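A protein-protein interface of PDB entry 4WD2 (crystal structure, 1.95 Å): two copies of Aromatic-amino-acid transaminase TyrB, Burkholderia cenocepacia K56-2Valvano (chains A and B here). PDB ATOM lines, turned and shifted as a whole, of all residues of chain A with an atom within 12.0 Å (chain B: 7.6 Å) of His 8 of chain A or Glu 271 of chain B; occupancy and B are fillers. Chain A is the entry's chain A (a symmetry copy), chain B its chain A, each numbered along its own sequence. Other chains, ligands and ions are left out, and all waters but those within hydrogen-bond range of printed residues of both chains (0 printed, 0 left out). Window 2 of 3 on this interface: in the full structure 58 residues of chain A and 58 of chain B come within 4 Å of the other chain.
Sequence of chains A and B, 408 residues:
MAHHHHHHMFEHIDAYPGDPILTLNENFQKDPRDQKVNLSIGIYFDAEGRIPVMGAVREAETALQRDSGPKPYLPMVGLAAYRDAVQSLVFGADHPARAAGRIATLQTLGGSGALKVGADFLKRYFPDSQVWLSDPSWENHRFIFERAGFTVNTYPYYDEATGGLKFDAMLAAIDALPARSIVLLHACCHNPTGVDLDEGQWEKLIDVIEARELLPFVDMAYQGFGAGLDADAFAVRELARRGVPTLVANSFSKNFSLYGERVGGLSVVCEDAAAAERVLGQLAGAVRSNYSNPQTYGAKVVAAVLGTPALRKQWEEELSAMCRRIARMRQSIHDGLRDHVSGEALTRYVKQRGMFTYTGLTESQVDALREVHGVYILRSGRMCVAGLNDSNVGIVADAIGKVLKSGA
His 8 of chain A touches one residue of chain B. Of the printed residues of chain B, Met 9 of chain A touches Phe 126 (3.6 Å), Glu 213 (3.6 Å), Pro 245 (3.7 Å) and Glu 271 (3.6 Å). Ile 103 of chain B touches none of the printed residues of chain A. Printed residues of chain A within 4 Å of Val 269 of chain B: Phe 10 (3.7 Å). Cys 270 of chain B touches just one residue of chain A: Phe 10. Of chain A, only His 8, Met 9, Phe 10 and Glu 11 come within 4 Å of Glu 271 of chain B. No residue of chain A comes within 4 Å of Ala 273 of chain B. No residue of chain A comes within 4 Å of Ala 275 of chain B. The nearest printed residue of chain B that does not touch His 8 of chain A is Pro 245 of chain B (6.9 Å).
Glu 271 of chain B touches His 8 of chain A (OE2 to C, 3.4 Å). CZ of Phe 126 of chain B touches O of Met 9 of chain A, at 3.6 Å. Met 9 of chain A touches Glu 213 of chain B. CB of Pro 245 of chain B touches CG of Met 9 of chain A, 3.7 Å away. Met 9 of chain A touches Glu 271 of chain B (N to OE2, 3.6 Å). Phe 10 of chain A touches Pro 245 of chain B. CZ of Phe 10 of chain A touches CG1 of Val 268 of chain B (3.8 Å). Phe 10 of chain A touches Val 269 of chain B (CE2 to O, 3.7 Å). SG of Cys 270 of chain B touches CD2 of Phe 10 of chain A, at 3.8 Å. Glu 11 of chain A touches Arg 278 of chain B.
Printed residues of chain A that touch a printed residue of chain B: His 8, Met 9, Phe 10, Glu 11 and Ile 13. Hydrophobic or aromatic side chains of chain A within 4 Å of the printed part of chain B: Met 9 and Phe 10. Of the 20 printed residues of chain B, 9 touch a printed residue of chain A. Among the printed residues, no Asp or Glu carboxylate lies within 4 Å of a Lys or Arg side-chain nitrogen of the other chain.
No position is printed for both chains. Of the 15 pairs that touch across the chains among the printed residues, none has its exchanged pair printed and touching as well.
The guanidinium group (NH2) of Arg 278 of chain B is in hydrogen-bond range of the backbone carbonyl oxygen (O) of Phe 10 of chain A, at 2.8 Å. OE2 of Glu 271 of chain B is in hydrogen-bond range of N of Phe 10 of chain A, 3.0 Å away. The backbone NH (N) of Glu 11 of chain A is in hydrogen-bond range of the side-chain carboxylate (OE2) of Glu 271 of chain B, 3.3 Å away. O of Ile 13 of chain A sits at hydrogen-bond distance from NE of Arg 278 of chain B (2.8 Å).
OE2 of Glu 11 of chain A lies within hydrogen-bond range of NE2 of His 12 of chain A (3.4 Å). The backbone NH (N) of Cys 270 of chain B sits at hydrogen-bond distance from the backbone carbonyl oxygen (O) of Arg 102 of chain B (2.7 Å). O of Val 268 of chain B sits at hydrogen-bond distance from SG of Cys 270 of chain B (3.8 Å).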
ATOM      1  N   HIS A   8      13.857  -9.145 -23.742  1.00  0.00           N
ATOM      2  CA  HIS A   8      13.276 -10.345 -24.329  1.00  0.00           C
ATOM      3  C   HIS A   8      13.604 -10.456 -25.816  1.00  0.00           C
ATOM      4  O   HIS A   8      12.854 -11.071 -26.573  1.00  0.00           O
ATOM      5  CB  HIS A   8      11.758 -10.352 -24.125  1.00  0.00           C
ATOM      6  N   MET A   9      14.728  -9.873 -26.228  1.00  0.00           N
ATOM      7  CA  MET A   9      15.080  -9.820 -27.647  1.00  0.00           C
ATOM      8  C   MET A   9      15.131 -11.211 -28.279  1.00  0.00           C
ATOM      9  O   MET A   9      14.691 -11.398 -29.411  1.00  0.00           O
ATOM     10  CB  MET A   9      16.424  -9.108 -27.852  1.00  0.00           C
ATOM     11  CG  MET A   9      16.870  -9.031 -29.311  1.00  0.00           C
ATOM     12  SD  MET A   9      15.815  -8.000 -30.368  1.00  0.00           S
ATOM     13  CE  MET A   9      16.177  -6.370 -29.713  1.00  0.00           C
ATOM     14  N   PHE A  10      15.643 -12.189 -27.542  1.00  0.00           N
ATOM     15  CA  PHE A  10      15.798 -13.531 -28.092  1.00  0.00           C
ATOM     16  C   PHE A  10      14.794 -14.528 -27.510  1.00  0.00           C
ATOM     17  O   PHE A  10      15.070 -15.724 -27.422  1.00  0.00           O
ATOM     18  CB  PHE A  10      17.229 -14.026 -27.871  1.00  0.00           C
ATOM     19  CG  PHE A  10      18.272 -13.143 -28.497  1.00  0.00           C
ATOM     20  CD1 PHE A  10      18.347 -13.013 -29.873  1.00  0.00           C
ATOM     21  CD2 PHE A  10      19.170 -12.434 -27.709  1.00  0.00           C
ATOM     22  CE1 PHE A  10      19.296 -12.196 -30.454  1.00  0.00           C
ATOM     23  CE2 PHE A  10      20.131 -11.610 -28.288  1.00  0.00           C
ATOM     24  CZ  PHE A  10      20.188 -11.493 -29.659  1.00  0.00           C
ATOM     25  N   GLU A  11      13.619 -14.043 -27.143  1.00  0.00           N
ATOM     26  CA  GLU A  11      12.622 -14.895 -26.506  1.00  0.00           C
ATOM     27  C   GLU A  11      12.029 -15.909 -27.485  1.00  0.00           C
ATOM     28  O   GLU A  11      11.437 -16.904 -27.069  1.00  0.00           O
ATOM     29  CB  GLU A  11      11.510 -14.040 -25.884  1.00  0.00           C
ATOM     30  CG  GLU A  11      10.650 -13.277 -26.885  1.00  0.00           C
ATOM     31  CD  GLU A  11       9.689 -12.307 -26.207  1.00  0.00           C
ATOM     32  OE1 GLU A  11       9.458 -12.456 -24.988  1.00  0.00           O
ATOM     33  OE2 GLU A  11       9.176 -11.392 -26.891  1.00  0.00           O
ATOM     34  N   HIS A  12      12.201 -15.669 -28.782  1.00  0.00           N
ATOM     35  CA  HIS A  12      11.588 -16.525 -29.791  1.00  0.00           C
ATOM     36  C   HIS A  12      12.594 -17.447 -30.461  1.00  0.00           C
ATOM     37  O   HIS A  12      12.236 -18.207 -31.360  1.00  0.00           O
ATOM     38  CB  HIS A  12      10.869 -15.681 -30.850  1.00  0.00           C
ATOM     39  CG  HIS A  12       9.742 -14.859 -30.304  1.00  0.00           C
ATOM     40  ND1 HIS A  12       8.632 -15.420 -29.710  1.00  0.00           N
ATOM     41  CD2 HIS A  12       9.556 -13.520 -30.258  1.00  0.00           C
ATOM     42  CE1 HIS A  12       7.810 -14.462 -29.325  1.00  0.00           C
ATOM     43  NE2 HIS A  12       8.347 -13.298 -29.644  1.00  0.00           N
ATOM     44  N   ILE A  13      13.851 -17.379 -30.031  1.00  0.00           N
ATOM     45  CA  ILE A  13      14.858 -18.312 -30.517  1.00  0.00           C
ATOM     46  C   ILE A  13      14.614 -19.694 -29.927  1.00  0.00           C
ATOM     47  O   ILE A  13      14.759 -19.905 -28.722  1.00  0.00           O
ATOM     48  CB  ILE A  13      16.286 -17.870 -30.160  1.00  0.00           C
ATOM     49  CG1 ILE A  13      16.493 -16.397 -30.497  1.00  0.00           C
ATOM     50  CG2 ILE A  13      17.292 -18.732 -30.907  1.00  0.00           C
ATOM     51  CD1 ILE A  13      16.342 -16.104 -31.947  1.00  0.00           C
ATOM     52  N   ASP A  14      14.242 -20.637 -30.781  1.00  0.00           N
ATOM     53  CA  ASP A  14      13.958 -21.983 -30.323  1.00  0.00           C
ATOM     54  C   ASP A  14      15.249 -22.731 -30.015  1.00  0.00           C
ATOM     55  O   ASP A  14      16.300 -22.452 -30.591  1.00  0.00           O
ATOM     56  CB  ASP A  14      13.120 -22.733 -31.358  1.00  0.00           C
ATOM     57  CG  ASP A  14      13.725 -22.689 -32.747  1.00  0.00           C
ATOM     58  OD1 ASP A  14      13.777 -21.595 -33.346  1.00  0.00           O
ATOM     59  OD2 ASP A  14      14.133 -23.756 -33.251  1.00  0.00           O
ATOM     60  N   ALA A  15      15.166 -23.667 -29.078  1.00  0.00           N
ATOM     61  CA  ALA A  15      16.310 -24.489 -28.710  1.00  0.00           C
ATOM     62  C   ALA A  15      16.688 -25.444 -29.843  1.00  0.00           C
ATOM     63  O   ALA A  15      15.822 -26.022 -30.496  1.00  0.00           O
ATOM     64  CB  ALA A  15      16.011 -25.263 -27.442  1.00  0.00           C
ATOM     65  N   ALA B 100      27.346 -14.482 -15.377  1.00  0.00           N
ATOM     66  CA  ALA B 100      25.931 -14.859 -15.353  1.00  0.00           C
ATOM     67  C   ALA B 100      25.533 -15.760 -16.528  1.00  0.00           C
ATOM     68  O   ALA B 100      24.356 -16.094 -16.698  1.00  0.00           O
ATOM     69  CB  ALA B 100      25.062 -13.617 -15.336  1.00  0.00           C
ATOM     70  N   GLY B 101      26.511 -16.156 -17.334  1.00  0.00           N
ATOM     71  CA  GLY B 101      26.255 -17.044 -18.455  1.00  0.00           C
ATOM     72  C   GLY B 101      25.360 -16.476 -19.546  1.00  0.00           C
ATOM     73  O   GLY B 101      24.679 -17.232 -20.252  1.00  0.00           O
ATOM     74  N   ARG B 102      25.369 -15.155 -19.691  1.00  0.00           N
ATOM     75  CA  ARG B 102      24.521 -14.474 -20.667  1.00  0.00           C
ATOM     76  C   ARG B 102      25.159 -14.325 -22.042  1.00  0.00           C
ATOM     77  O   ARG B 102      24.572 -13.706 -22.927  1.00  0.00           O
ATOM     78  CB  ARG B 102      24.141 -13.085 -20.157  1.00  0.00           C
ATOM     79  CG  ARG B 102      23.180 -13.078 -18.991  1.00  0.00           C
ATOM     80  CD  ARG B 102      22.676 -11.667 -18.718  1.00  0.00           C
ATOM     81  NE  ARG B 102      23.684 -10.816 -18.080  1.00  0.00           N
ATOM     82  CZ  ARG B 102      23.731 -10.569 -16.772  1.00  0.00           C
ATOM     83  NH1 ARG B 102      22.826 -11.108 -15.962  1.00  0.00           N
ATOM     84  NH2 ARG B 102      24.679  -9.780 -16.272  1.00  0.00           N
ATOM     85  N   ILE B 103      26.357 -14.875 -22.224  1.00  0.00           N
ATOM     86  CA  ILE B 103      27.081 -14.721 -23.488  1.00  0.00           C
ATOM     87  C   ILE B 103      27.300 -16.047 -24.207  1.00  0.00           C
ATOM     88  O   ILE B 103      27.957 -16.935 -23.679  1.00  0.00           O
ATOM     89  CB  ILE B 103      28.466 -14.076 -23.279  1.00  0.00           C
ATOM     90  CG1 ILE B 103      28.363 -12.768 -22.499  1.00  0.00           C
ATOM     91  CG2 ILE B 103      29.147 -13.821 -24.618  1.00  0.00           C
ATOM     92  CD1 ILE B 103      29.723 -12.196 -22.148  1.00  0.00           C
ATOM     93  N   PHE B 126      15.251 -12.773 -37.597  1.00  0.00           N
ATOM     94  CA  PHE B 126      14.796 -11.398 -37.791  1.00  0.00           C
ATOM     95  C   PHE B 126      14.749 -11.029 -39.280  1.00  0.00           C
ATOM     96  O   PHE B 126      15.408 -10.082 -39.709  1.00  0.00           O
ATOM     97  CB  PHE B 126      15.710 -10.432 -37.028  1.00  0.00           C
ATOM     98  CG  PHE B 126      15.798 -10.719 -35.548  1.00  0.00           C
ATOM     99  CD1 PHE B 126      14.936 -10.097 -34.659  1.00  0.00           C
ATOM    100  CD2 PHE B 126      16.730 -11.624 -35.052  1.00  0.00           C
ATOM    101  CE1 PHE B 126      15.007 -10.362 -33.293  1.00  0.00           C
ATOM    102  CE2 PHE B 126      16.808 -11.897 -33.694  1.00  0.00           C
ATOM    103  CZ  PHE B 126      15.952 -11.262 -32.811  1.00  0.00           C
ATOM    104  N   GLU B 213      15.397  -0.293 -28.905  1.00  0.00           N
ATOM    105  CA  GLU B 213      15.370  -1.749 -29.039  1.00  0.00           C
ATOM    106  C   GLU B 213      16.015  -2.201 -30.334  1.00  0.00           C
ATOM    107  O   GLU B 213      15.483  -3.059 -31.044  1.00  0.00           O
ATOM    108  CB  GLU B 213      13.931  -2.279 -28.964  1.00  0.00           C
ATOM    109  CG  GLU B 213      13.265  -2.017 -27.628  1.00  0.00           C
ATOM    110  CD  GLU B 213      11.799  -2.375 -27.636  1.00  0.00           C
ATOM    111  OE1 GLU B 213      10.979  -1.487 -27.334  1.00  0.00           O
ATOM    112  OE2 GLU B 213      11.465  -3.539 -27.946  1.00  0.00           O
ATOM    113  N   GLY B 243      23.159  -4.694 -20.355  1.00  0.00           N
ATOM    114  CA  GLY B 243      22.198  -5.723 -20.717  1.00  0.00           C
ATOM    115  C   GLY B 243      21.614  -5.623 -22.115  1.00  0.00           C
ATOM    116  O   GLY B 243      20.553  -6.181 -22.392  1.00  0.00           O
ATOM    117  N   VAL B 244      22.297  -4.919 -23.006  1.00  0.00           N
ATOM    118  CA  VAL B 244      21.793  -4.722 -24.362  1.00  0.00           C
ATOM    119  C   VAL B 244      22.085  -5.946 -25.231  1.00  0.00           C
ATOM    120  O   VAL B 244      23.214  -6.440 -25.240  1.00  0.00           O
ATOM    121  CB  VAL B 244      22.410  -3.451 -25.000  1.00  0.00           C
ATOM    122  CG1 VAL B 244      21.923  -3.264 -26.433  1.00  0.00           C
ATOM    123  CG2 VAL B 244      22.070  -2.222 -24.156  1.00  0.00           C
ATOM    124  N   PRO B 245      21.060  -6.456 -25.946  1.00  0.00           N
ATOM    125  CA  PRO B 245      21.255  -7.548 -26.909  1.00  0.00           C
ATOM    126  C   PRO B 245      22.297  -7.178 -27.951  1.00  0.00           C
ATOM    127  O   PRO B 245      22.042  -6.304 -28.776  1.00  0.00           O
ATOM    128  CB  PRO B 245      19.872  -7.707 -27.559  1.00  0.00           C
ATOM    129  CG  PRO B 245      19.165  -6.393 -27.285  1.00  0.00           C
ATOM    130  CD  PRO B 245      19.658  -6.002 -25.916  1.00  0.00           C
ATOM    131  N   VAL B 268      27.369 -13.479 -28.661  1.00  0.00           N
ATOM    132  CA  VAL B 268      26.065 -12.838 -28.569  1.00  0.00           C
ATOM    133  C   VAL B 268      25.671 -12.705 -27.097  1.00  0.00           C
ATOM    134  O   VAL B 268      25.687 -13.689 -26.352  1.00  0.00           O
ATOM    135  CB  VAL B 268      24.996 -13.624 -29.354  1.00  0.00           C
ATOM    136  CG1 VAL B 268      23.662 -12.888 -29.328  1.00  0.00           C
ATOM    137  CG2 VAL B 268      25.453 -13.841 -30.789  1.00  0.00           C
ATOM    138  N   VAL B 269      25.346 -11.480 -26.685  1.00  0.00           N
ATOM    139  CA  VAL B 269      24.949 -11.193 -25.311  1.00  0.00           C
ATOM    140  C   VAL B 269      23.436 -11.232 -25.197  1.00  0.00           C
ATOM    141  O   VAL B 269      22.743 -10.476 -25.877  1.00  0.00           O
ATOM    142  CB  VAL B 269      25.453  -9.817 -24.857  1.00  0.00           C
ATOM    143  CG1 VAL B 269      25.101  -9.571 -23.394  1.00  0.00           C
ATOM    144  CG2 VAL B 269      26.951  -9.690 -25.089  1.00  0.00           C
ATOM    145  N   CYS B 270      22.921 -12.103 -24.332  1.00  0.00           N
ATOM    146  CA  CYS B 270      21.482 -12.372 -24.277  1.00  0.00           C
ATOM    147  C   CYS B 270      20.868 -11.999 -22.928  1.00  0.00           C
ATOM    148  O   CYS B 270      21.588 -11.703 -21.975  1.00  0.00           O
ATOM    149  CB  CYS B 270      21.212 -13.849 -24.579  1.00  0.00           C
ATOM    150  SG  CYS B 270      21.975 -14.428 -26.110  1.00  0.00           S
ATOM    151  N   GLU B 271      19.538 -12.024 -22.848  1.00  0.00           N
ATOM    152  CA  GLU B 271      18.837 -11.535 -21.663  1.00  0.00           C
ATOM    153  C   GLU B 271      19.046 -12.421 -20.429  1.00  0.00           C
ATOM    154  O   GLU B 271      19.000 -11.927 -19.300  1.00  0.00           O
ATOM    155  CB  GLU B 271      17.337 -11.371 -21.953  1.00  0.00           C
ATOM    156  CG  GLU B 271      16.646 -12.596 -22.538  1.00  0.00           C
ATOM    157  CD  GLU B 271      16.590 -12.592 -24.064  1.00  0.00           C
ATOM    158  OE1 GLU B 271      17.585 -12.196 -24.713  1.00  0.00           O
ATOM    159  OE2 GLU B 271      15.540 -12.991 -24.612  1.00  0.00           O
ATOM    160  N   ASP B 272      19.263 -13.719 -20.629  1.00  0.00           N
ATOM    161  CA  ASP B 272      19.656 -14.603 -19.524  1.00  0.00           C
ATOM    162  C   ASP B 272      20.404 -15.833 -20.037  1.00  0.00           C
ATOM    163  O   ASP B 272      20.570 -16.006 -21.246  1.00  0.00           O
ATOM    164  CB  ASP B 272      18.440 -15.024 -18.677  1.00  0.00           C
ATOM    165  CG  ASP B 272      17.364 -15.742 -19.479  1.00  0.00           C
ATOM    166  OD1 ASP B 272      17.660 -16.286 -20.562  1.00  0.00           O
ATOM    167  OD2 ASP B 272      16.209 -15.778 -19.003  1.00  0.00           O
ATOM    168  N   ALA B 273      20.857 -16.684 -19.122  1.00  0.00           N
ATOM    169  CA  ALA B 273      21.662 -17.842 -19.503  1.00  0.00           C
ATOM    170  C   ALA B 273      20.868 -18.829 -20.356  1.00  0.00           C
ATOM    171  O   ALA B 273      21.420 -19.465 -21.252  1.00  0.00           O
ATOM    172  CB  ALA B 273      22.210 -18.531 -18.277  1.00  0.00           C
ATOM    173  N   ALA B 274      19.576 -18.956 -20.068  1.00  0.00           N
ATOM    174  CA  ALA B 274      18.709 -19.848 -20.823  1.00  0.00           C
ATOM    175  C   ALA B 274      18.677 -19.409 -22.283  1.00  0.00           C
ATOM    176  O   ALA B 274      18.885 -20.217 -23.187  1.00  0.00           O
ATOM    177  CB  ALA B 274      17.310 -19.865 -20.230  1.00  0.00           C
ATOM    178  N   ALA B 275      18.444 -18.119 -22.499  1.00  0.00           N
ATOM    179  CA  ALA B 275      18.438 -17.550 -23.843  1.00  0.00           C
ATOM    180  C   ALA B 275      19.788 -17.728 -24.546  1.00  0.00           C
ATOM    181  O   ALA B 275      19.833 -18.060 -25.736  1.00  0.00           O
ATOM    182  CB  ALA B 275      18.057 -16.066 -23.788  1.00  0.00           C
ATOM    183  N   ALA B 276      20.879 -17.507 -23.815  1.00  0.00           N
ATOM    184  CA  ALA B 276      22.221 -17.638 -24.378  1.00  0.00           C
ATOM    185  C   ALA B 276      22.478 -19.047 -24.906  1.00  0.00           C
ATOM    186  O   ALA B 276      23.136 -19.225 -25.934  1.00  0.00           O
ATOM    187  CB  ALA B 276      23.269 -17.271 -23.338  1.00  0.00           C
ATOM    188  N   ARG B 278      20.097 -21.202 -25.943  1.00  0.00           N
ATOM    189  CA  ARG B 278      19.268 -21.427 -27.125  1.00  0.00           C
ATOM    190  C   ARG B 278      19.925 -20.757 -28.325  1.00  0.00           C
ATOM    191  O   ARG B 278      19.976 -21.328 -29.419  1.00  0.00           O
ATOM    192  CB  ARG B 278      17.844 -20.894 -26.938  1.00  0.00           C
ATOM    193  CG  ARG B 278      17.071 -21.555 -25.806  1.00  0.00           C
ATOM    194  CD  ARG B 278      15.588 -21.202 -25.850  1.00  0.00           C
ATOM    195  NE  ARG B 278      15.351 -19.770 -26.038  1.00  0.00           N
ATOM    196  CZ  ARG B 278      15.217 -18.888 -25.053  1.00  0.00           C
ATOM    197  NH1 ARG B 278      15.299 -19.275 -23.785  1.00  0.00           N
ATOM    198  NH2 ARG B 278      15.009 -17.611 -25.333  1.00  0.00           N
ATOM    199  N   VAL B 279      20.436 -19.548 -28.116  1.00  0.00           N
ATOM    200  CA  VAL B 279      21.119 -18.827 -29.181  1.00  0.00           C
ATOM    201  C   VAL B 279      22.368 -19.592 -29.629  1.00  0.00           C
ATOM    202  O   VAL B 279      22.597 -19.743 -30.827  1.00  0.00           O
ATOM    203  CB  VAL B 279      21.487 -17.396 -28.752  1.00  0.00           C
ATOM    204  CG1 VAL B 279      22.521 -16.793 -29.688  1.00  0.00           C
ATOM    205  CG2 VAL B 279      20.239 -16.530 -28.708  1.00  0.00           C
